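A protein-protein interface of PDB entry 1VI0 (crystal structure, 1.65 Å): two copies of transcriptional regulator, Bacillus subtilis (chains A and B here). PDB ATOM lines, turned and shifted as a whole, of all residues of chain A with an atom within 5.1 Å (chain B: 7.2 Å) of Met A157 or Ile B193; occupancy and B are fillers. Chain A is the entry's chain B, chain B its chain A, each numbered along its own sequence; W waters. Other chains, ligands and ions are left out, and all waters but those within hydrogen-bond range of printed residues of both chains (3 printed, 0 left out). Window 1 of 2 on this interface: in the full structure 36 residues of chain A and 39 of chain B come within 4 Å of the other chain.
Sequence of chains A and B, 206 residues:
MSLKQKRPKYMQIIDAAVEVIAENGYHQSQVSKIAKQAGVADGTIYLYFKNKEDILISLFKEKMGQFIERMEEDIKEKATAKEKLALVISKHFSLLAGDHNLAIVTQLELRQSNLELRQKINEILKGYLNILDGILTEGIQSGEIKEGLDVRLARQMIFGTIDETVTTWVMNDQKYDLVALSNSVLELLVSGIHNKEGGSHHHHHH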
ATOM      1  N   LEU A  85     -11.049  -7.044  24.538  1.00  0.00           N
ATOM      2  CA  LEU A  85     -12.513  -6.864  24.653  1.00  0.00           C
ATOM      3  C   LEU A  85     -12.825  -5.696  25.612  1.00  0.00           C
ATOM      4  O   LEU A  85     -13.775  -4.941  25.419  1.00  0.00           O
ATOM      5  CB  LEU A  85     -13.095  -8.133  25.268  1.00  0.00           C
ATOM      6  CG  LEU A  85     -14.609  -8.173  25.509  1.00  0.00           C
ATOM      7  CD1 LEU A  85     -15.387  -7.539  24.359  1.00  0.00           C
ATOM      8  CD2 LEU A  85     -15.035  -9.624  25.724  1.00  0.00           C
ATOM      9  N   LEU A 136     -11.681 -13.506  19.717  1.00  0.00           N
ATOM     10  CA  LEU A 136     -12.061 -14.825  20.212  1.00  0.00           C
ATOM     11  C   LEU A 136     -11.179 -15.920  19.564  1.00  0.00           C
ATOM     12  O   LEU A 136     -10.666 -16.769  20.278  1.00  0.00           O
ATOM     13  CB  LEU A 136     -13.522 -15.135  19.887  1.00  0.00           C
ATOM     14  CG  LEU A 136     -14.547 -14.227  20.626  1.00  0.00           C
ATOM     15  CD1 LEU A 136     -15.879 -14.345  19.952  1.00  0.00           C
ATOM     16  CD2 LEU A 136     -14.569 -14.552  22.123  1.00  0.00           C
ATOM     17  N   GLU A 144      -6.513 -18.722  26.400  1.00  0.00           N
ATOM     18  CA  GLU A 144      -7.220 -17.830  27.301  1.00  0.00           C
ATOM     19  C   GLU A 144      -8.751 -18.047  27.199  1.00  0.00           C
ATOM     20  O   GLU A 144      -9.386 -18.001  28.278  1.00  0.00           O
ATOM     21  CB  GLU A 144      -6.915 -16.385  27.003  1.00  0.00           C
ATOM     22  CG  GLU A 144      -7.829 -15.479  27.873  1.00  0.00           C
ATOM     23  CD  GLU A 144      -7.578 -14.033  27.470  1.00  0.00           C
ATOM     24  OE1 GLU A 144      -6.899 -13.894  26.417  1.00  0.00           O
ATOM     25  OE2 GLU A 144      -8.073 -13.170  28.184  1.00  0.00           O
ATOM     26  N   ILE A 145      -9.214 -18.354  26.018  1.00  0.00           N
ATOM     27  CA  ILE A 145     -10.651 -18.517  25.756  1.00  0.00           C
ATOM     28  C   ILE A 145     -11.015 -20.005  25.706  1.00  0.00           C
ATOM     29  O   ILE A 145     -10.223 -20.850  25.272  1.00  0.00           O
ATOM     30  CB  ILE A 145     -11.081 -17.815  24.465  1.00  0.00           C
ATOM     31  CG1 ILE A 145     -10.877 -16.292  24.476  1.00  0.00           C
ATOM     32  CG2 ILE A 145     -12.545 -18.108  24.102  1.00  0.00           C
ATOM     33  CD1 ILE A 145     -11.611 -15.526  25.547  1.00  0.00           C
ATOM     34  N   LYS A 146     -12.218 -20.301  26.192  1.00  0.00           N
ATOM     35  CA  LYS A 146     -12.749 -21.672  26.201  1.00  0.00           C
ATOM     36  C   LYS A 146     -12.452 -22.486  24.959  1.00  0.00           C
ATOM     37  O   LYS A 146     -12.780 -22.094  23.839  1.00  0.00           O
ATOM     38  CB  LYS A 146     -14.296 -21.513  26.337  1.00  0.00           C
ATOM     39  CG  LYS A 146     -15.000 -22.682  26.903  1.00  0.00           C
ATOM     40  CD  LYS A 146     -16.399 -22.409  27.410  1.00  0.00           C
ATOM     41  CE  LYS A 146     -16.405 -21.451  28.582  1.00  0.00           C
ATOM     42  NZ  LYS A 146     -16.382 -22.081  29.915  1.00  0.00           N
ATOM     43  N   LEU A 149     -15.087 -23.328  21.890  1.00  0.00           N
ATOM     44  CA  LEU A 149     -16.053 -22.204  21.785  1.00  0.00           C
ATOM     45  C   LEU A 149     -16.506 -21.983  20.340  1.00  0.00           C
ATOM     46  O   LEU A 149     -15.688 -22.100  19.403  1.00  0.00           O
ATOM     47  CB  LEU A 149     -15.277 -20.907  22.143  1.00  0.00           C
ATOM     48  CG  LEU A 149     -16.148 -19.645  22.265  1.00  0.00           C
ATOM     49  CD1 LEU A 149     -16.441 -19.309  23.715  1.00  0.00           C
ATOM     50  CD2 LEU A 149     -15.427 -18.493  21.588  1.00  0.00           C
ATOM     51  N   LEU A 153     -21.262 -17.923  17.641  1.00  0.00           N
ATOM     52  CA  LEU A 153     -22.243 -17.772  18.723  1.00  0.00           C
ATOM     53  C   LEU A 153     -21.704 -16.851  19.837  1.00  0.00           C
ATOM     54  O   LEU A 153     -22.521 -16.032  20.322  1.00  0.00           O
ATOM     55  CB  LEU A 153     -22.572 -19.106  19.364  1.00  0.00           C
ATOM     56  CG  LEU A 153     -23.552 -20.042  18.657  1.00  0.00           C
ATOM     57  CD1 LEU A 153     -23.827 -21.226  19.605  1.00  0.00           C
ATOM     58  CD2 LEU A 153     -24.845 -19.345  18.320  1.00  0.00           C
ATOM     59  N   ALA A 154     -20.448 -16.963  20.187  1.00  0.00           N
ATOM     60  CA  ALA A 154     -19.885 -16.127  21.269  1.00  0.00           C
ATOM     61  C   ALA A 154     -19.825 -14.664  20.851  1.00  0.00           C
ATOM     62  O   ALA A 154     -20.097 -13.724  21.634  1.00  0.00           O
ATOM     63  CB  ALA A 154     -18.534 -16.585  21.729  1.00  0.00           C
ATOM     64  N   ARG A 155     -19.584 -14.445  19.548  1.00  0.00           N
ATOM     65  CA  ARG A 155     -19.671 -13.076  19.029  1.00  0.00           C
ATOM     66  C   ARG A 155     -21.098 -12.566  19.069  1.00  0.00           C
ATOM     67  O   ARG A 155     -21.307 -11.368  19.412  1.00  0.00           O
ATOM     68  CB  ARG A 155     -19.086 -13.034  17.622  1.00  0.00           C
ATOM     69  CG  ARG A 155     -19.523 -11.781  16.858  1.00  0.00           C
ATOM     70  CD  ARG A 155     -20.447 -12.113  15.727  1.00  0.00           C
ATOM     71  NE  ARG A 155     -19.744 -12.891  14.655  1.00  0.00           N
ATOM     72  CZ  ARG A 155     -20.286 -13.495  13.646  1.00  0.00           C
ATOM     73  NH1 ARG A 155     -21.590 -13.545  13.368  1.00  0.00           N
ATOM     74  NH2 ARG A 155     -19.450 -14.152  12.780  1.00  0.00           N
ATOM     75  N   GLN A 156     -22.113 -13.414  18.829  1.00  0.00           N
ATOM     76  CA  GLN A 156     -23.517 -12.968  18.929  1.00  0.00           C
ATOM     77  C   GLN A 156     -23.789 -12.609  20.421  1.00  0.00           C
ATOM     78  O   GLN A 156     -24.518 -11.624  20.625  1.00  0.00           O
ATOM     79  CB  GLN A 156     -24.423 -14.033  18.349  1.00  0.00           C
ATOM     80  CG  GLN A 156     -24.278 -14.165  16.791  1.00  0.00           C
ATOM     81  CD  GLN A 156     -24.891 -15.448  16.287  1.00  0.00           C
ATOM     82  OE1 GLN A 156     -26.074 -15.790  16.477  1.00  0.00           O
ATOM     83  NE2 GLN A 156     -24.087 -16.328  15.589  1.00  0.00           N
ATOM     84  N   MET A 157     -23.307 -13.415  21.359  1.00  0.00           N
ATOM     85  CA  MET A 157     -23.524 -13.038  22.764  1.00  0.00           C
ATOM     86  C   MET A 157     -22.784 -11.740  23.097  1.00  0.00           C
ATOM     87  O   MET A 157     -23.441 -10.828  23.703  1.00  0.00           O
ATOM     88  CB  MET A 157     -22.966 -14.150  23.706  1.00  0.00           C
ATOM     89  CG  MET A 157     -23.124 -13.652  25.173  1.00  0.00           C
ATOM     90  SD  MET A 157     -22.451 -15.025  26.469  1.00  0.00           S
ATOM     91  CE  MET A 157     -20.729 -14.994  25.597  1.00  0.00           C
ATOM     92  N   ILE A 158     -21.570 -11.518  22.660  1.00  0.00           N
ATOM     93  CA  ILE A 158     -20.855 -10.274  23.047  1.00  0.00           C
ATOM     94  C   ILE A 158     -21.524  -9.079  22.412  1.00  0.00           C
ATOM     95  O   ILE A 158     -21.936  -8.107  23.116  1.00  0.00           O
ATOM     96  CB  ILE A 158     -19.364 -10.404  22.687  1.00  0.00           C
ATOM     97  CG1 ILE A 158     -18.708 -11.531  23.510  1.00  0.00           C
ATOM     98  CG2 ILE A 158     -18.640  -9.070  22.862  1.00  0.00           C
ATOM     99  CD1 ILE A 158     -17.353 -11.954  22.989  1.00  0.00           C
ATOM    100  N   PHE A 159     -21.737  -9.084  21.098  1.00  0.00           N
ATOM    101  CA  PHE A 159     -22.440  -8.021  20.416  1.00  0.00           C
ATOM    102  C   PHE A 159     -23.862  -7.799  20.884  1.00  0.00           C
ATOM    103  O   PHE A 159     -24.226  -6.648  21.286  1.00  0.00           O
ATOM    104  CB  PHE A 159     -22.352  -8.196  18.879  1.00  0.00           C
ATOM    105  CG  PHE A 159     -22.954  -6.928  18.260  1.00  0.00           C
ATOM    106  CD1 PHE A 159     -24.270  -6.915  17.844  1.00  0.00           C
ATOM    107  CD2 PHE A 159     -22.203  -5.785  18.246  1.00  0.00           C
ATOM    108  CE1 PHE A 159     -24.807  -5.736  17.332  1.00  0.00           C
ATOM    109  CE2 PHE A 159     -22.748  -4.602  17.726  1.00  0.00           C
ATOM    110  CZ  PHE A 159     -24.066  -4.596  17.295  1.00  0.00           C
ATOM    111  N   GLY A 160     -24.606  -8.832  21.246  1.00  0.00           N
ATOM    112  CA  GLY A 160     -26.000  -8.729  21.682  1.00  0.00           C
ATOM    113  C   GLY A 160     -26.067  -8.038  23.092  1.00  0.00           C
ATOM    114  O   GLY A 160     -26.965  -7.234  23.304  1.00  0.00           O
ATOM    115  N   THR A 161     -25.117  -8.402  23.913  1.00  0.00           N
ATOM    116  CA  THR A 161     -24.964  -7.933  25.303  1.00  0.00           C
ATOM    117  C   THR A 161     -24.611  -6.441  25.262  1.00  0.00           C
ATOM    118  O   THR A 161     -25.273  -5.650  25.899  1.00  0.00           O
ATOM    119  CB  THR A 161     -23.982  -8.716  26.128  1.00  0.00           C
ATOM    120  OG1 THR A 161     -24.450 -10.071  26.276  1.00  0.00           O
ATOM    121  CG2 THR A 161     -23.739  -8.103  27.526  1.00  0.00           C
ATOM    122  N   ILE A 162     -23.547  -6.108  24.544  1.00  0.00           N
ATOM    123  CA  ILE A 162     -23.209  -4.683  24.353  1.00  0.00           C
ATOM    124  C   ILE A 162     -24.391  -3.910  23.842  1.00  0.00           C
ATOM    125  O   ILE A 162     -24.841  -2.864  24.437  1.00  0.00           O
ATOM    126  CB  ILE A 162     -22.017  -4.592  23.364  1.00  0.00           C
ATOM    127  CG1 ILE A 162     -20.773  -5.246  23.984  1.00  0.00           C
ATOM    128  CG2 ILE A 162     -21.847  -3.128  22.968  1.00  0.00           C
ATOM    129  CD1 ILE A 162     -19.584  -5.290  22.971  1.00  0.00           C
ATOM    130  N   LEU A 189     -19.521 -11.316  30.615  1.00  0.00           N
ATOM    131  CA  LEU A 189     -19.214 -12.094  29.384  1.00  0.00           C
ATOM    132  C   LEU A 189     -18.101 -13.068  29.645  1.00  0.00           C
ATOM    133  O   LEU A 189     -18.173 -14.159  29.059  1.00  0.00           O
ATOM    134  CB  LEU A 189     -18.830 -11.079  28.288  1.00  0.00           C
ATOM    135  CG  LEU A 189     -20.029 -10.234  27.801  1.00  0.00           C
ATOM    136  CD1 LEU A 189     -19.556  -9.052  26.975  1.00  0.00           C
ATOM    137  CD2 LEU A 189     -21.054 -11.036  26.988  1.00  0.00           C
ATOM    138  N   VAL A 190     -17.091 -12.684  30.400  1.00  0.00           N
ATOM    139  CA  VAL A 190     -15.917 -13.563  30.606  1.00  0.00           C
ATOM    140  C   VAL A 190     -16.252 -14.731  31.503  1.00  0.00           C
ATOM    141  O   VAL A 190     -15.813 -15.884  31.279  1.00  0.00           O
ATOM    142  CB  VAL A 190     -14.769 -12.729  31.211  1.00  0.00           C
ATOM    143  CG1 VAL A 190     -13.641 -13.588  31.735  1.00  0.00           C
ATOM    144  CG2 VAL A 190     -14.253 -11.698  30.200  1.00  0.00           C
ATOM    145  N   SER A 191     -17.029 -14.489  32.571  1.00  0.00           N
ATOM    146  CA  SER A 191     -17.331 -15.499  33.567  1.00  0.00           C
ATOM    147  C   SER A 191     -18.761 -15.992  33.671  1.00  0.00           C
ATOM    148  O   SER A 191     -18.942 -17.080  34.301  1.00  0.00           O
ATOM    149  CB  SER A 191     -16.918 -14.935  34.978  1.00  0.00           C
ATOM    150  OG  SER A 191     -15.484 -14.938  34.971  1.00  0.00           O
ATOM    151  N   GLN B 156     -29.898  -7.904  30.927  1.00  0.00           N
ATOM    152  CA  GLN B 156     -29.585  -7.272  29.601  1.00  0.00           C
ATOM    153  C   GLN B 156     -28.686  -8.235  28.840  1.00  0.00           C
ATOM    154  O   GLN B 156     -28.854  -8.357  27.608  1.00  0.00           O
ATOM    155  CB  GLN B 156     -28.956  -5.918  29.928  1.00  0.00           C
ATOM    156  CG  GLN B 156     -30.125  -4.994  30.371  1.00  0.00           C
ATOM    157  CD  GLN B 156     -29.626  -3.770  31.132  1.00  0.00           C
ATOM    158  OE1 GLN B 156     -28.528  -3.244  30.964  1.00  0.00           O
ATOM    159  NE2 GLN B 156     -30.565  -3.178  31.896  1.00  0.00           N
ATOM    160  N   MET B 157     -27.728  -8.827  29.496  1.00  0.00           N
ATOM    161  CA  MET B 157     -26.863  -9.829  28.808  1.00  0.00           C
ATOM    162  C   MET B 157     -27.718 -10.982  28.330  1.00  0.00           C
ATOM    163  O   MET B 157     -27.590 -11.418  27.120  1.00  0.00           O
ATOM    164  CB  MET B 157     -25.753 -10.302  29.718  1.00  0.00           C
ATOM    165  CG  MET B 157     -24.822 -11.329  29.139  1.00  0.00           C
ATOM    166  SD  MET B 157     -23.314 -12.102  29.977  1.00  0.00           S
ATOM    167  CE  MET B 157     -24.062 -13.094  31.435  1.00  0.00           C
ATOM    168  N   ILE B 158     -28.576 -11.556  29.150  1.00  0.00           N
ATOM    169  CA  ILE B 158     -29.364 -12.724  28.749  1.00  0.00           C
ATOM    170  C   ILE B 158     -30.268 -12.426  27.598  1.00  0.00           C
ATOM    171  O   ILE B 158     -30.291 -13.048  26.532  1.00  0.00           O
ATOM    172  CB  ILE B 158     -30.166 -13.321  29.945  1.00  0.00           C
ATOM    173  CG1 ILE B 158     -29.147 -13.811  30.977  1.00  0.00           C
ATOM    174  CG2 ILE B 158     -31.107 -14.381  29.469  1.00  0.00           C
ATOM    175  CD1 ILE B 158     -29.803 -14.178  32.300  1.00  0.00           C
ATOM    176  N   GLY B 160     -30.134  -9.759  25.586  1.00  0.00           N
ATOM    177  CA  GLY B 160     -29.443  -9.256  24.336  1.00  0.00           C
ATOM    178  C   GLY B 160     -28.798 -10.448  23.601  1.00  0.00           C
ATOM    179  O   GLY B 160     -28.830 -10.403  22.362  1.00  0.00           O
ATOM    180  N   THR B 161     -28.290 -11.419  24.329  1.00  0.00           N
ATOM    181  CA  THR B 161     -27.652 -12.612  23.708  1.00  0.00           C
ATOM    182  C   THR B 161     -28.711 -13.434  22.981  1.00  0.00           C
ATOM    183  O   THR B 161     -28.599 -13.716  21.786  1.00  0.00           O
ATOM    184  CB  THR B 161     -26.961 -13.433  24.798  1.00  0.00           C
ATOM    185  OG1 THR B 161     -25.839 -12.685  25.306  1.00  0.00           O
ATOM    186  CG2 THR B 161     -26.490 -14.796  24.284  1.00  0.00           C
ATOM    187  N   ILE B 162     -29.862 -13.696  23.599  1.00  0.00           N
ATOM    188  CA  ILE B 162     -30.947 -14.405  22.996  1.00  0.00           C
ATOM    189  C   ILE B 162     -31.445 -13.729  21.715  1.00  0.00           C
ATOM    190  O   ILE B 162     -31.487 -14.211  20.562  1.00  0.00           O
ATOM    191  CB  ILE B 162     -32.125 -14.618  23.969  1.00  0.00           C
ATOM    192  CG1 ILE B 162     -31.698 -15.494  25.175  1.00  0.00           C
ATOM    193  CG2 ILE B 162     -33.270 -15.304  23.225  1.00  0.00           C
ATOM    194  CD1 ILE B 162     -32.783 -15.566  26.283  1.00  0.00           C
ATOM    195  N   GLU B 164     -29.940 -11.308  19.961  1.00  0.00           N
ATOM    196  CA  GLU B 164     -28.986 -11.118  18.809  1.00  0.00           C
ATOM    197  C   GLU B 164     -28.840 -12.473  18.092  1.00  0.00           C
ATOM    198  O   GLU B 164     -28.597 -12.455  16.860  1.00  0.00           O
ATOM    199  CB  GLU B 164     -27.645 -10.619  19.320  1.00  0.00           C
ATOM    200  CG  GLU B 164     -26.568 -10.512  18.250  1.00  0.00           C
ATOM    201  CD  GLU B 164     -26.920  -9.477  17.176  1.00  0.00           C
ATOM    202  OE1 GLU B 164     -27.765  -8.611  17.398  1.00  0.00           O
ATOM    203  OE2 GLU B 164     -26.312  -9.635  16.082  1.00  0.00           O
ATOM    204  N   THR B 165     -28.948 -13.547  18.853  1.00  0.00           N
ATOM    205  CA  THR B 165     -28.913 -14.881  18.176  1.00  0.00           C
ATOM    206  C   THR B 165     -30.051 -15.005  17.198  1.00  0.00           C
ATOM    207  O   THR B 165     -29.873 -15.413  16.003  1.00  0.00           O
ATOM    208  CB  THR B 165     -28.828 -16.027  19.203  1.00  0.00           C
ATOM    209  OG1 THR B 165     -27.678 -15.858  20.031  1.00  0.00           O
ATOM    210  CG2 THR B 165     -28.614 -17.325  18.378  1.00  0.00           C
ATOM    211  N   VAL B 185     -26.140 -21.751  23.615  1.00  0.00           N
ATOM    212  CA  VAL B 185     -26.379 -20.327  24.012  1.00  0.00           C
ATOM    213  C   VAL B 185     -26.485 -20.291  25.553  1.00  0.00           C
ATOM    214  O   VAL B 185     -25.755 -19.523  26.187  1.00  0.00           O
ATOM    215  CB  VAL B 185     -27.661 -19.827  23.375  1.00  0.00           C
ATOM    216  CG1 VAL B 185     -27.922 -18.412  23.966  1.00  0.00           C
ATOM    217  CG2 VAL B 185     -27.453 -19.621  21.858  1.00  0.00           C
ATOM    218  N   LEU B 186     -27.289 -21.201  26.074  1.00  0.00           N
ATOM    219  CA  LEU B 186     -27.322 -21.369  27.561  1.00  0.00           C
ATOM    220  C   LEU B 186     -25.963 -21.503  28.168  1.00  0.00           C
ATOM    221  O   LEU B 186     -25.592 -20.775  29.137  1.00  0.00           O
ATOM    222  CB  LEU B 186     -28.162 -22.642  27.863  1.00  0.00           C
ATOM    223  CG  LEU B 186     -28.116 -23.033  29.342  1.00  0.00           C
ATOM    224  CD1 LEU B 186     -28.926 -22.045  30.217  1.00  0.00           C
ATOM    225  CD2 LEU B 186     -28.717 -24.422  29.492  1.00  0.00           C
ATOM    226  N   GLU B 187     -25.071 -22.435  27.694  1.00  0.00           N
ATOM    227  CA  GLU B 187     -23.769 -22.620  28.285  1.00  0.00           C
ATOM    228  C   GLU B 187     -22.869 -21.391  28.219  1.00  0.00           C
ATOM    229  O   GLU B 187     -22.057 -21.139  29.149  1.00  0.00           O
ATOM    230  CB  GLU B 187     -23.107 -23.885  27.701  1.00  0.00           C
ATOM    231  CG  GLU B 187     -23.844 -25.173  28.135  1.00  0.00           C
ATOM    232  CD  GLU B 187     -23.810 -25.354  29.656  1.00  0.00           C
ATOM    233  OE1 GLU B 187     -22.962 -24.752  30.333  1.00  0.00           O
ATOM    234  OE2 GLU B 187     -24.629 -26.147  30.168  1.00  0.00           O
ATOM    235  N   LEU B 188     -22.969 -20.610  27.150  1.00  0.00           N
ATOM    236  CA  LEU B 188     -22.235 -19.376  26.998  1.00  0.00           C
ATOM    237  C   LEU B 188     -22.692 -18.387  28.105  1.00  0.00           C
ATOM    238  O   LEU B 188     -21.788 -17.788  28.702  1.00  0.00           O
ATOM    239  CB  LEU B 188     -22.496 -18.700  25.631  1.00  0.00           C
ATOM    240  CG  LEU B 188     -21.635 -19.411  24.486  1.00  0.00           C
ATOM    241  CD1 LEU B 188     -22.186 -19.110  23.153  1.00  0.00           C
ATOM    242  CD2 LEU B 188     -20.198 -18.936  24.694  1.00  0.00           C
ATOM    243  N   LEU B 189     -23.974 -18.287  28.388  1.00  0.00           N
ATOM    244  CA  LEU B 189     -24.477 -17.360  29.430  1.00  0.00           C
ATOM    245  C   LEU B 189     -24.078 -17.847  30.825  1.00  0.00           C
ATOM    246  O   LEU B 189     -23.666 -17.043  31.680  1.00  0.00           O
ATOM    247  CB  LEU B 189     -26.007 -17.237  29.318  1.00  0.00           C
ATOM    248  CG  LEU B 189     -26.531 -16.511  28.034  1.00  0.00           C
ATOM    249  CD1 LEU B 189     -27.991 -16.679  27.843  1.00  0.00           C
ATOM    250  CD2 LEU B 189     -26.132 -15.026  28.120  1.00  0.00           C
ATOM    251  N   VAL B 190     -24.085 -19.154  31.046  1.00  0.00           N
ATOM    252  CA  VAL B 190     -23.787 -19.784  32.313  1.00  0.00           C
ATOM    253  C   VAL B 190     -22.330 -19.696  32.680  1.00  0.00           C
ATOM    254  O   VAL B 190     -22.036 -19.350  33.819  1.00  0.00           O
ATOM    255  CB  VAL B 190     -24.355 -21.225  32.364  1.00  0.00           C
ATOM    256  CG1 VAL B 190     -23.756 -21.974  33.550  1.00  0.00           C
ATOM    257  CG2 VAL B 190     -25.858 -21.208  32.377  1.00  0.00           C
ATOM    258  N   SER B 191     -21.384 -19.914  31.755  1.00  0.00           N
ATOM    259  CA  SER B 191     -19.961 -19.971  32.060  1.00  0.00           C
ATOM    260  C   SER B 191     -19.114 -18.942  31.346  1.00  0.00           C
ATOM    261  O   SER B 191     -17.898 -18.882  31.654  1.00  0.00           O
ATOM    262  CB  SER B 191     -19.392 -21.387  31.737  1.00  0.00           C
ATOM    263  OG  SER B 191     -20.123 -22.366  32.474  1.00  0.00           O
ATOM    264  N   GLY B 192     -19.627 -18.188  30.410  1.00  0.00           N
ATOM    265  CA  GLY B 192     -18.934 -17.126  29.733  1.00  0.00           C
ATOM    266  C   GLY B 192     -17.861 -17.674  28.785  1.00  0.00           C
ATOM    267  O   GLY B 192     -17.891 -18.886  28.507  1.00  0.00           O
ATOM    268  N   ILE B 193     -16.966 -16.819  28.286  1.00  0.00           N
ATOM    269  CA  ILE B 193     -15.968 -17.275  27.304  1.00  0.00           C
ATOM    270  C   ILE B 193     -14.644 -17.670  27.906  1.00  0.00           C
ATOM    271  O   ILE B 193     -13.771 -18.225  27.186  1.00  0.00           O
ATOM    272  CB  ILE B 193     -15.713 -16.148  26.256  1.00  0.00           C
ATOM    273  CG1 ILE B 193     -14.979 -14.986  26.909  1.00  0.00           C
ATOM    274  CG2 ILE B 193     -17.018 -15.718  25.575  1.00  0.00           C
ATOM    275  CD1 ILE B 193     -14.819 -13.749  26.047  1.00  0.00           C
ATOM    276  N   HIS B 194     -14.368 -17.464  29.176  1.00  0.00           N
ATOM    277  CA  HIS B 194     -13.061 -17.763  29.765  1.00  0.00           C
ATOM    278  C   HIS B 194     -12.691 -19.242  29.663  1.00  0.00           C
ATOM    279  O   HIS B 194     -13.594 -20.089  29.796  1.00  0.00           O
ATOM    280  CB  HIS B 194     -13.041 -17.371  31.247  1.00  0.00           C
ATOM    281  CG  HIS B 194     -13.758 -18.343  32.139  1.00  0.00           C
ATOM    282  ND1 HIS B 194     -15.122 -18.489  32.191  1.00  0.00           N
ATOM    283  CD2 HIS B 194     -13.247 -19.240  33.035  1.00  0.00           C
ATOM    284  CE1 HIS B 194     -15.433 -19.436  33.065  1.00  0.00           C
ATOM    285  NE2 HIS B 194     -14.323 -19.909  33.592  1.00  0.00           N
ATOM    286  N   ASN B 195     -11.413 -19.539  29.550  1.00  0.00           N
ATOM    287  CA  ASN B 195     -10.982 -20.963  29.518  1.00  0.00           C
ATOM    288  C   ASN B 195     -10.993 -21.527  30.941  1.00  0.00           C
ATOM    289  O   ASN B 195     -10.618 -20.824  31.881  1.00  0.00           O
ATOM    290  CB  ASN B 195      -9.587 -21.118  28.950  1.00  0.00           C
ATOM    291  CG  ASN B 195      -9.122 -22.532  28.705  1.00  0.00           C
ATOM    292  OD1 ASN B 195      -9.156 -23.421  29.558  1.00  0.00           O
ATOM    293  ND2 ASN B 195      -8.651 -22.795  27.476  1.00  0.00           N
ATOM    294  N   LYS B 196     -11.300 -22.800  31.076  1.00  0.00           N
ATOM    295  CA  LYS B 196     -11.317 -23.565  32.299  1.00  0.00           C
ATOM    296  C   LYS B 196     -12.769 -23.877  32.709  1.00  0.00           C
ATOM    297  O   LYS B 196     -13.672 -23.253  32.119  1.00  0.00           O
ATOM    298  CB  LYS B 196     -10.551 -22.962  33.450  1.00  0.00           C
ATOM    299  CG  LYS B 196      -9.036 -23.044  33.407  1.00  0.00           C
ATOM    300  CD  LYS B 196      -8.407 -21.784  34.010  1.00  0.00           C
ATOM    301  CE  LYS B 196      -6.907 -21.930  34.171  1.00  0.00           C
ATOM    302  NZ  LYS B 196      -6.210 -22.193  32.871  1.00  0.00           N
HETATM  303  O   HOH W   1     -25.205 -16.673  21.338  1.00  0.00           O
HETATM  304  O   HOH W   2      -9.878 -17.470  31.090  1.00  0.00           O
HETATM  305  O   HOH W   3     -27.881 -17.228  15.198  1.00  0.00           O
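The side-chain hydroxyl (OG1) of Thr B161 lies close to the backbone carbonyl oxygen (O) of Met A157 (3.4 Å).
The side-chain hydroxyl (OG1) of Thr A161 lies within hydrogen-bond range of the side-chain hydroxyl (OG1) of Thr B161 (3.1 Å).
O of Ile B193 lies within hydrogen-bond range of N of Lys A146, 2.8 Å away.
The backbone NH (N) of Ile B193 is in hydrogen-bond range of the backbone carbonyl oxygen (O) of Leu A189, 3.0 Å away.
O of Val A190 sits at hydrogen-bond distance from N of Ile B193, 3.3 Å away.
The backbone carbonyl oxygen (O) of His B194 sits close to the side-chain amino group (NZ) of Lys A146, 3.4 Å away.
A ring nitrogen (ND1) of His B194 lies within hydrogen-bond range of the backbone carbonyl oxygen (O) of Val A190, 2.8 Å away.
O of Glu A144 lies within hydrogen-bond range of N of Asn B195 (2.8 Å).
O of Ile A145 lies within hydrogen-bond range of ND2 of Asn B195 (3.3 Å).
SD of Met A157 sits close to O of Leu B188.
O of Ser A191 sits close to O of Ser B191, 3.4 Å away.
The side-chain hydroxyl of Thr B161 is in hydrogen-bond range of the backbone carbonyl oxygen of Met B157.
A ring nitrogen (ND1) of His B194 lies within hydrogen-bond range of the backbone carbonyl oxygen of Ser B191.
O of Met A157 lies within hydrogen-bond range of OG1 of Thr A161 (2.9 Å).
Ile A145 touches Ile B193.
Lys A146 touches Ser B191.
Lys A146 touches Asn B195 (N to N, 3.5 Å).
CG of Glu B164 touches O of Gln A156 (3.3 Å).
CB of Glu B164 touches CA of Gly A160, at 3.4 Å.
O of Leu A189 touches CA of Gly B192 (3.1 Å).
Ser A191 touches Val B190 (O to O, 3.9 Å).
Of chain B, only Thr B161 (2.9 Å), Leu B188 (3.6 Å) and Ile B193 (3.8 Å) come within 4 Å of Met A157.
Of the printed residues of chain A, Ile B193 touches Ile A145, Lys A146, Met A157, Leu A189 and Val A190.
Of the printed residues of chain A, Gly B160 touches Gly A160.
Of the printed residues of chain B, Gln A156 touches Glu B164 (3.3 Å) and Thr B165 (3.4 Å).
Leu B189 touches none of the printed residues of chain A.
The nearest printed residue of chain A that does not touch Ile B193 is Leu A136 (4.01 Å).
Of the 20 printed residues of chain B, 13 touch a printed residue of chain A.
Printed residues of chain A that touch a printed residue of chain B: Glu A144, Ile A145, Lys A146, Leu A149, Leu A153, Gln A156, Met A157, Phe A159, Gly A160, Thr A161, Leu A189, Val A190 and Ser A191.
Along chain A the printed residues that touch a printed residue of chain B span positions 144 to 191.
Gly B160 touches its own counterpart, Gly A160.
Leu A189 touches Met B157, but with the chains exchanged Met A157 does not touch Leu B189 (4.03 Å).
Val A190 touches Ser B191, and with the chains exchanged Ser A191 touches Val B190.
Ser B191 touches its own counterpart, Ser A191.
Water W3 bridges OE1 of Gln A156 and O of Thr B165.
Water W2 lies within hydrogen-bond range of the backbone carbonyl oxygen (O) of Glu A144 and the backbone NH (N) of Asn B195.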
